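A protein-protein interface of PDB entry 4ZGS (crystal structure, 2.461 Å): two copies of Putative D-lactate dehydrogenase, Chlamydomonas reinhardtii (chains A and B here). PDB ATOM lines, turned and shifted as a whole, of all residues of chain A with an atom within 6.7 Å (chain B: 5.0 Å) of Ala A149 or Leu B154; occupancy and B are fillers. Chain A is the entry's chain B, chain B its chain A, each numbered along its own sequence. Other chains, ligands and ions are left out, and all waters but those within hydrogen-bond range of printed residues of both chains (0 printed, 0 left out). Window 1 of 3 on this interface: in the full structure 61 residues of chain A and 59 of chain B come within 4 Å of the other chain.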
ATOM      1  N   HIS A 142      -9.379  21.893   9.508  1.00  0.00           N
ATOM      2  CA  HIS A 142     -10.781  21.505   9.546  1.00  0.00           C
ATOM      3  C   HIS A 142     -11.372  21.802  10.922  1.00  0.00           C
ATOM      4  O   HIS A 142     -12.480  22.336  11.041  1.00  0.00           O
ATOM      5  CB  HIS A 142     -10.964  20.029   9.224  1.00  0.00           C
ATOM      6  CG  HIS A 142     -12.399  19.629   9.105  1.00  0.00           C
ATOM      7  ND1 HIS A 142     -13.140  19.848   7.962  1.00  0.00           N
ATOM      8  CD2 HIS A 142     -13.244  19.058   9.996  1.00  0.00           C
ATOM      9  CE1 HIS A 142     -14.371  19.415   8.151  1.00  0.00           C
ATOM     10  NE2 HIS A 142     -14.466  18.945   9.382  1.00  0.00           N
ATOM     11  N   VAL A 144     -10.295  24.115  12.729  1.00  0.00           N
ATOM     12  CA  VAL A 144     -10.451  25.557  12.780  1.00  0.00           C
ATOM     13  C   VAL A 144     -11.725  25.978  11.994  1.00  0.00           C
ATOM     14  O   VAL A 144     -12.542  26.752  12.516  1.00  0.00           O
ATOM     15  CB  VAL A 144      -9.144  26.257  12.292  1.00  0.00           C
ATOM     16  CG1 VAL A 144      -9.302  27.734  12.136  1.00  0.00           C
ATOM     17  CG2 VAL A 144      -8.059  25.972  13.277  1.00  0.00           C
ATOM     18  N   ALA A 145     -11.965  25.377  10.830  1.00  0.00           N
ATOM     19  CA  ALA A 145     -13.186  25.650  10.061  1.00  0.00           C
ATOM     20  C   ALA A 145     -14.430  25.386  10.929  1.00  0.00           C
ATOM     21  O   ALA A 145     -15.366  26.165  10.931  1.00  0.00           O
ATOM     22  CB  ALA A 145     -13.231  24.791   8.782  1.00  0.00           C
ATOM     23  N   LEU A 146     -14.441  24.297  11.686  1.00  0.00           N
ATOM     24  CA  LEU A 146     -15.591  24.034  12.547  1.00  0.00           C
ATOM     25  C   LEU A 146     -15.829  25.176  13.509  1.00  0.00           C
ATOM     26  O   LEU A 146     -16.968  25.677  13.645  1.00  0.00           O
ATOM     27  CB  LEU A 146     -15.416  22.710  13.312  1.00  0.00           C
ATOM     28  CG  LEU A 146     -15.514  21.384  12.522  1.00  0.00           C
ATOM     29  CD1 LEU A 146     -15.413  20.154  13.435  1.00  0.00           C
ATOM     30  CD2 LEU A 146     -16.852  21.355  11.844  1.00  0.00           C
ATOM     31  N   ILE A 147     -14.748  25.639  14.138  1.00  0.00           N
ATOM     32  CA  ILE A 147     -14.872  26.682  15.124  1.00  0.00           C
ATOM     33  C   ILE A 147     -15.465  27.922  14.462  1.00  0.00           C
ATOM     34  O   ILE A 147     -16.394  28.540  14.972  1.00  0.00           O
ATOM     35  CB  ILE A 147     -13.512  26.995  15.771  1.00  0.00           C
ATOM     36  CG1 ILE A 147     -13.146  25.864  16.724  1.00  0.00           C
ATOM     37  CG2 ILE A 147     -13.576  28.323  16.556  1.00  0.00           C
ATOM     38  CD1 ILE A 147     -11.725  25.919  17.171  1.00  0.00           C
ATOM     39  N   PHE A 148     -14.939  28.263  13.298  1.00  0.00           N
ATOM     40  CA  PHE A 148     -15.404  29.438  12.604  1.00  0.00           C
ATOM     41  C   PHE A 148     -16.906  29.301  12.228  1.00  0.00           C
ATOM     42  O   PHE A 148     -17.682  30.228  12.459  1.00  0.00           O
ATOM     43  CB  PHE A 148     -14.507  29.677  11.382  1.00  0.00           C
ATOM     44  CG  PHE A 148     -13.378  30.651  11.644  1.00  0.00           C
ATOM     45  CD1 PHE A 148     -13.589  32.016  11.572  1.00  0.00           C
ATOM     46  CD2 PHE A 148     -12.124  30.198  12.038  1.00  0.00           C
ATOM     47  CE1 PHE A 148     -12.558  32.904  11.821  1.00  0.00           C
ATOM     48  CE2 PHE A 148     -11.098  31.089  12.297  1.00  0.00           C
ATOM     49  CZ  PHE A 148     -11.329  32.447  12.195  1.00  0.00           C
ATOM     50  N   ALA A 149     -17.319  28.136  11.706  1.00  0.00           N
ATOM     51  CA  ALA A 149     -18.695  27.967  11.250  1.00  0.00           C
ATOM     52  C   ALA A 149     -19.646  28.123  12.443  1.00  0.00           C
ATOM     53  O   ALA A 149     -20.611  28.851  12.359  1.00  0.00           O
ATOM     54  CB  ALA A 149     -18.902  26.597  10.545  1.00  0.00           C
ATOM     55  N   LEU A 150     -19.350  27.472  13.561  1.00  0.00           N
ATOM     56  CA  LEU A 150     -20.189  27.604  14.754  1.00  0.00           C
ATOM     57  C   LEU A 150     -20.197  29.023  15.322  1.00  0.00           C
ATOM     58  O   LEU A 150     -21.231  29.487  15.815  1.00  0.00           O
ATOM     59  CB  LEU A 150     -19.708  26.657  15.843  1.00  0.00           C
ATOM     60  CG  LEU A 150     -19.911  25.196  15.500  1.00  0.00           C
ATOM     61  CD1 LEU A 150     -19.080  24.351  16.440  1.00  0.00           C
ATOM     62  CD2 LEU A 150     -21.424  24.832  15.560  1.00  0.00           C
ATOM     63  N   ASN A 151     -19.030  29.681  15.331  1.00  0.00           N
ATOM     64  CA  ASN A 151     -18.963  31.041  15.875  1.00  0.00           C
ATOM     65  C   ASN A 151     -19.931  31.971  15.173  1.00  0.00           C
ATOM     66  O   ASN A 151     -20.520  32.880  15.786  1.00  0.00           O
ATOM     67  CB  ASN A 151     -17.581  31.654  15.714  1.00  0.00           C
ATOM     68  CG  ASN A 151     -16.630  31.286  16.813  1.00  0.00           C
ATOM     69  OD1 ASN A 151     -17.013  30.823  17.887  1.00  0.00           O
ATOM     70  ND2 ASN A 151     -15.357  31.523  16.550  1.00  0.00           N
ATOM     71  N   ARG A 152     -19.976  31.811  13.854  1.00  0.00           N
ATOM     72  CA  ARG A 152     -20.741  32.706  12.999  1.00  0.00           C
ATOM     73  C   ARG A 152     -22.063  32.062  12.519  1.00  0.00           C
ATOM     74  O   ARG A 152     -22.684  32.554  11.586  1.00  0.00           O
ATOM     75  CB  ARG A 152     -19.863  33.221  11.858  1.00  0.00           C
ATOM     76  CG  ARG A 152     -18.479  33.868  12.371  1.00  0.00           C
ATOM     77  CD  ARG A 152     -18.644  34.916  13.491  1.00  0.00           C
ATOM     78  NE  ARG A 152     -19.241  36.075  12.863  1.00  0.00           N
ATOM     79  CZ  ARG A 152     -18.597  37.150  12.460  1.00  0.00           C
ATOM     80  NH1 ARG A 152     -17.282  37.297  12.679  1.00  0.00           N
ATOM     81  NH2 ARG A 152     -19.295  38.102  11.859  1.00  0.00           N
ATOM     82  N   HIS A 153     -22.431  30.921  13.086  1.00  0.00           N
ATOM     83  CA  HIS A 153     -23.705  30.276  12.720  1.00  0.00           C
ATOM     84  C   HIS A 153     -23.883  30.161  11.221  1.00  0.00           C
ATOM     85  O   HIS A 153     -24.896  30.585  10.689  1.00  0.00           O
ATOM     86  CB  HIS A 153     -24.913  31.029  13.308  1.00  0.00           C
ATOM     87  CG  HIS A 153     -24.918  31.092  14.797  1.00  0.00           C
ATOM     88  ND1 HIS A 153     -24.397  32.161  15.502  1.00  0.00           N
ATOM     89  CD2 HIS A 153     -25.367  30.213  15.726  1.00  0.00           C
ATOM     90  CE1 HIS A 153     -24.535  31.940  16.798  1.00  0.00           C
ATOM     91  NE2 HIS A 153     -25.127  30.769  16.963  1.00  0.00           N
ATOM     92  N   LEU A 154     -22.849  29.702  10.538  1.00  0.00           N
ATOM     93  CA  LEU A 154     -22.873  29.639   9.085  1.00  0.00           C
ATOM     94  C   LEU A 154     -23.909  28.664   8.519  1.00  0.00           C
ATOM     95  O   LEU A 154     -24.549  28.998   7.516  1.00  0.00           O
ATOM     96  CB  LEU A 154     -21.492  29.288   8.543  1.00  0.00           C
ATOM     97  CG  LEU A 154     -20.495  30.401   8.856  1.00  0.00           C
ATOM     98  CD1 LEU A 154     -19.111  30.185   8.176  1.00  0.00           C
ATOM     99  CD2 LEU A 154     -21.131  31.687   8.405  1.00  0.00           C
ATOM    100  N   THR A 155     -24.108  27.512   9.166  1.00  0.00           N
ATOM    101  CA  THR A 155     -25.038  26.539   8.628  1.00  0.00           C
ATOM    102  C   THR A 155     -26.483  27.090   8.694  1.00  0.00           C
ATOM    103  O   THR A 155     -27.187  27.096   7.668  1.00  0.00           O
ATOM    104  CB  THR A 155     -24.933  25.165   9.352  1.00  0.00           C
ATOM    105  OG1 THR A 155     -25.249  25.304  10.740  1.00  0.00           O
ATOM    106  CG2 THR A 155     -23.534  24.564   9.212  1.00  0.00           C
ATOM    107  N   LEU A 331     -22.521  20.935  15.450  1.00  0.00           N
ATOM    108  CA  LEU A 331     -22.171  20.846  14.053  1.00  0.00           C
ATOM    109  C   LEU A 331     -21.336  19.587  13.876  1.00  0.00           C
ATOM    110  O   LEU A 331     -20.377  19.387  14.600  1.00  0.00           O
ATOM    111  CB  LEU A 331     -21.412  22.083  13.589  1.00  0.00           C
ATOM    112  CG  LEU A 331     -20.854  21.985  12.178  1.00  0.00           C
ATOM    113  CD1 LEU A 331     -21.908  21.394  11.288  1.00  0.00           C
ATOM    114  CD2 LEU A 331     -20.497  23.340  11.652  1.00  0.00           C
ATOM    115  N   VAL A 332     -21.764  18.699  12.983  1.00  0.00           N
ATOM    116  CA  VAL A 332     -21.110  17.420  12.786  1.00  0.00           C
ATOM    117  C   VAL A 332     -20.794  17.224  11.312  1.00  0.00           C
ATOM    118  O   VAL A 332     -21.690  17.355  10.471  1.00  0.00           O
ATOM    119  CB  VAL A 332     -21.976  16.230  13.252  1.00  0.00           C
ATOM    120  CG1 VAL A 332     -21.304  14.920  12.832  1.00  0.00           C
ATOM    121  CG2 VAL A 332     -22.176  16.244  14.749  1.00  0.00           C
ATOM    122  N   THR A 333     -19.537  16.899  11.004  1.00  0.00           N
ATOM    123  CA  THR A 333     -19.145  16.539   9.643  1.00  0.00           C
ATOM    124  C   THR A 333     -18.826  15.042   9.593  1.00  0.00           C
ATOM    125  O   THR A 333     -18.461  14.447  10.620  1.00  0.00           O
ATOM    126  CB  THR A 333     -17.926  17.359   9.127  1.00  0.00           C
ATOM    127  OG1 THR A 333     -16.854  17.335  10.096  1.00  0.00           O
ATOM    128  CG2 THR A 333     -18.321  18.792   8.828  1.00  0.00           C
ATOM    129  N   THR A 336     -14.635  14.037   7.606  1.00  0.00           N
ATOM    130  CA  THR A 336     -13.953  14.671   6.485  1.00  0.00           C
ATOM    131  C   THR A 336     -12.691  15.468   6.870  1.00  0.00           C
ATOM    132  O   THR A 336     -12.095  16.104   6.007  1.00  0.00           O
ATOM    133  CB  THR A 336     -14.884  15.613   5.733  1.00  0.00           C
ATOM    134  OG1 THR A 336     -15.220  16.716   6.571  1.00  0.00           O
ATOM    135  CG2 THR A 336     -16.142  14.881   5.289  1.00  0.00           C
ATOM    136  N   PHE B 148     -13.170  29.353   5.188  1.00  0.00           N
ATOM    137  CA  PHE B 148     -13.063  28.018   5.728  1.00  0.00           C
ATOM    138  C   PHE B 148     -14.241  27.137   5.335  1.00  0.00           C
ATOM    139  O   PHE B 148     -14.033  26.007   4.934  1.00  0.00           O
ATOM    140  CB  PHE B 148     -12.900  28.070   7.245  1.00  0.00           C
ATOM    141  CG  PHE B 148     -11.448  28.053   7.681  1.00  0.00           C
ATOM    142  CD1 PHE B 148     -10.728  26.871   7.701  1.00  0.00           C
ATOM    143  CD2 PHE B 148     -10.806  29.224   8.051  1.00  0.00           C
ATOM    144  CE1 PHE B 148      -9.422  26.861   8.105  1.00  0.00           C
ATOM    145  CE2 PHE B 148      -9.503  29.208   8.443  1.00  0.00           C
ATOM    146  CZ  PHE B 148      -8.813  28.028   8.467  1.00  0.00           C
ATOM    147  N   ALA B 149     -15.462  27.675   5.421  1.00  0.00           N
ATOM    148  CA  ALA B 149     -16.665  26.921   5.178  1.00  0.00           C
ATOM    149  C   ALA B 149     -16.649  26.421   3.733  1.00  0.00           C
ATOM    150  O   ALA B 149     -16.881  25.245   3.487  1.00  0.00           O
ATOM    151  CB  ALA B 149     -17.933  27.783   5.474  1.00  0.00           C
ATOM    152  N   ARG B 152     -13.966  23.654   3.013  1.00  0.00           N
ATOM    153  CA  ARG B 152     -14.284  22.362   3.567  1.00  0.00           C
ATOM    154  C   ARG B 152     -15.710  21.931   3.287  1.00  0.00           C
ATOM    155  O   ARG B 152     -16.155  20.947   3.871  1.00  0.00           O
ATOM    156  CB  ARG B 152     -13.971  22.349   5.057  1.00  0.00           C
ATOM    157  CG  ARG B 152     -12.498  22.745   5.338  1.00  0.00           C
ATOM    158  CD  ARG B 152     -11.501  21.922   4.466  1.00  0.00           C
ATOM    159  NE  ARG B 152     -11.361  20.531   4.913  1.00  0.00           N
ATOM    160  CZ  ARG B 152     -10.347  20.065   5.644  1.00  0.00           C
ATOM    161  NH1 ARG B 152      -9.349  20.879   6.018  1.00  0.00           N
ATOM    162  NH2 ARG B 152     -10.330  18.777   6.010  1.00  0.00           N
ATOM    163  N   HIS B 153     -16.435  22.685   2.453  1.00  0.00           N
ATOM    164  CA  HIS B 153     -17.816  22.335   2.093  1.00  0.00           C
ATOM    165  C   HIS B 153     -18.657  22.087   3.327  1.00  0.00           C
ATOM    166  O   HIS B 153     -19.441  21.127   3.370  1.00  0.00           O
ATOM    167  CB  HIS B 153     -17.879  21.048   1.191  1.00  0.00           C
ATOM    168  CG  HIS B 153     -17.159  21.164  -0.112  1.00  0.00           C
ATOM    169  ND1 HIS B 153     -17.731  21.727  -1.233  1.00  0.00           N
ATOM    170  CD2 HIS B 153     -15.910  20.788  -0.482  1.00  0.00           C
ATOM    171  CE1 HIS B 153     -16.870  21.684  -2.239  1.00  0.00           C
ATOM    172  NE2 HIS B 153     -15.757  21.120  -1.810  1.00  0.00           N
ATOM    173  N   LEU B 154     -18.526  22.948   4.321  1.00  0.00           N
ATOM    174  CA  LEU B 154     -19.270  22.771   5.566  1.00  0.00           C
ATOM    175  C   LEU B 154     -20.805  22.845   5.396  1.00  0.00           C
ATOM    176  O   LEU B 154     -21.517  22.104   6.081  1.00  0.00           O
ATOM    177  CB  LEU B 154     -18.828  23.800   6.623  1.00  0.00           C
ATOM    178  CG  LEU B 154     -17.377  23.722   7.112  1.00  0.00           C
ATOM    179  CD1 LEU B 154     -17.186  24.642   8.354  1.00  0.00           C
ATOM    180  CD2 LEU B 154     -16.965  22.314   7.430  1.00  0.00           C
ATOM    181  N   THR B 155     -21.343  23.704   4.522  1.00  0.00           N
ATOM    182  CA  THR B 155     -22.816  23.751   4.428  1.00  0.00           C
ATOM    183  C   THR B 155     -23.378  22.464   3.789  1.00  0.00           C
ATOM    184  O   THR B 155     -24.265  21.832   4.361  1.00  0.00           O
ATOM    185  CB  THR B 155     -23.336  24.997   3.655  1.00  0.00           C
ATOM    186  OG1 THR B 155     -22.935  24.958   2.276  1.00  0.00           O
ATOM    187  CG2 THR B 155     -22.844  26.312   4.336  1.00  0.00           C
ATOM    188  N   ASP B 156     -22.833  22.044   2.653  1.00  0.00           N
ATOM    189  CA  ASP B 156     -23.154  20.724   2.105  1.00  0.00           C
ATOM    190  C   ASP B 156     -23.035  19.628   3.170  1.00  0.00           C
ATOM    191  O   ASP B 156     -23.931  18.798   3.307  1.00  0.00           O
ATOM    192  CB  ASP B 156     -22.251  20.367   0.921  1.00  0.00           C
ATOM    193  CG  ASP B 156     -22.476  21.257  -0.291  1.00  0.00           C
ATOM    194  OD1 ASP B 156     -23.302  22.200  -0.209  1.00  0.00           O
ATOM    195  OD2 ASP B 156     -21.801  21.020  -1.323  1.00  0.00           O
ATOM    196  N   ALA B 157     -21.927  19.603   3.915  1.00  0.00           N
ATOM    197  CA  ALA B 157     -21.703  18.499   4.840  1.00  0.00           C
ATOM    198  C   ALA B 157     -22.750  18.432   5.921  1.00  0.00           C
ATOM    199  O   ALA B 157     -23.264  17.364   6.245  1.00  0.00           O
ATOM    200  CB  ALA B 157     -20.348  18.610   5.459  1.00  0.00           C
ATOM    201  N   TYR B 158     -23.065  19.592   6.475  1.00  0.00           N
ATOM    202  CA  TYR B 158     -24.033  19.702   7.546  1.00  0.00           C
ATOM    203  C   TYR B 158     -25.379  19.136   7.091  1.00  0.00           C
ATOM    204  O   TYR B 158     -26.006  18.361   7.822  1.00  0.00           O
ATOM    205  CB  TYR B 158     -24.156  21.160   8.002  1.00  0.00           C
ATOM    206  CG  TYR B 158     -25.210  21.374   9.054  1.00  0.00           C
ATOM    207  CD1 TYR B 158     -25.027  20.905  10.357  1.00  0.00           C
ATOM    208  CD2 TYR B 158     -26.385  22.043   8.753  1.00  0.00           C
ATOM    209  CE1 TYR B 158     -26.002  21.078  11.327  1.00  0.00           C
ATOM    210  CE2 TYR B 158     -27.348  22.234   9.724  1.00  0.00           C
ATOM    211  CZ  TYR B 158     -27.152  21.743  11.001  1.00  0.00           C
ATOM    212  OH  TYR B 158     -28.121  21.935  11.951  1.00  0.00           O
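Of the printed residues of chain B, Val A144 touches Phe B148 (3.7 Å). Ala A149 touches one residue of chain B. Asn A151 touches none of the printed residues of chain B. Printed residues of chain B within 4 Å of Leu A154: Ala B149. Printed residues of chain B within 4 Å of Leu A331: Tyr B158 (3.3 Å). Leu B154 touches three residues of chain A. Of the printed residues of chain A, Tyr B158 touches Thr A155 (3.5 Å) and Leu A331 (3.3 Å). The nearest printed residue of chain B that does not touch Ala A149 is Ala B149 (5.3 Å). The nearest printed residue of chain B that does not touch Thr A336 is Ala B157 (5.6 Å).
Of the 17 printed residues of chain A, 9 touch a printed residue of chain B. Printed residues of chain B that touch a printed residue of chain A: Phe B148, Ala B149, Arg B152, Leu B154, Ala B157 and Tyr B158. Among the printed residues, no Asp or Glu carboxylate lies within 4 Å of a Lys or Arg side-chain nitrogen of the other chain.
The backbone carbonyl oxygen (O) of Thr A336 lies within hydrogen-bond range of the guanidinium group (NH2) of Arg B152 (3.2 Å).
Ala A149 touches Leu B154, and with the chains exchanged Leu A154 touches Ala B149. Positions printed for both chains: 148, 149, 152, 153, 154 and 155. Of the 11 pairs that touch across the chains among the printed residues, 2 have their exchanged pair printed and touching as well.
The backbone carbonyl oxygen of Ala B149 lies within hydrogen-bond range of the backbone NH of Leu B154 (2.9 Å). OG1 of Thr A333 sits at hydrogen-bond distance from NE2 of His A142. The backbone NH (N) of Leu A154 sits at hydrogen-bond distance from the backbone carbonyl oxygen (O) of Ala A149, 3.0 Å away.
Among the printed residues, pairs that only touch across the chains: His A142 with Arg B152, His A142 with Leu B154, Val A144 with Phe B148, Ala A145 with Phe B148, Ala A145 with Leu B154, Ala A149 with Leu B154, Leu A154 with Ala B149, Thr A155 with Tyr B158, Leu A331 with Tyr B158 and Thr A333 with Ala B157.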
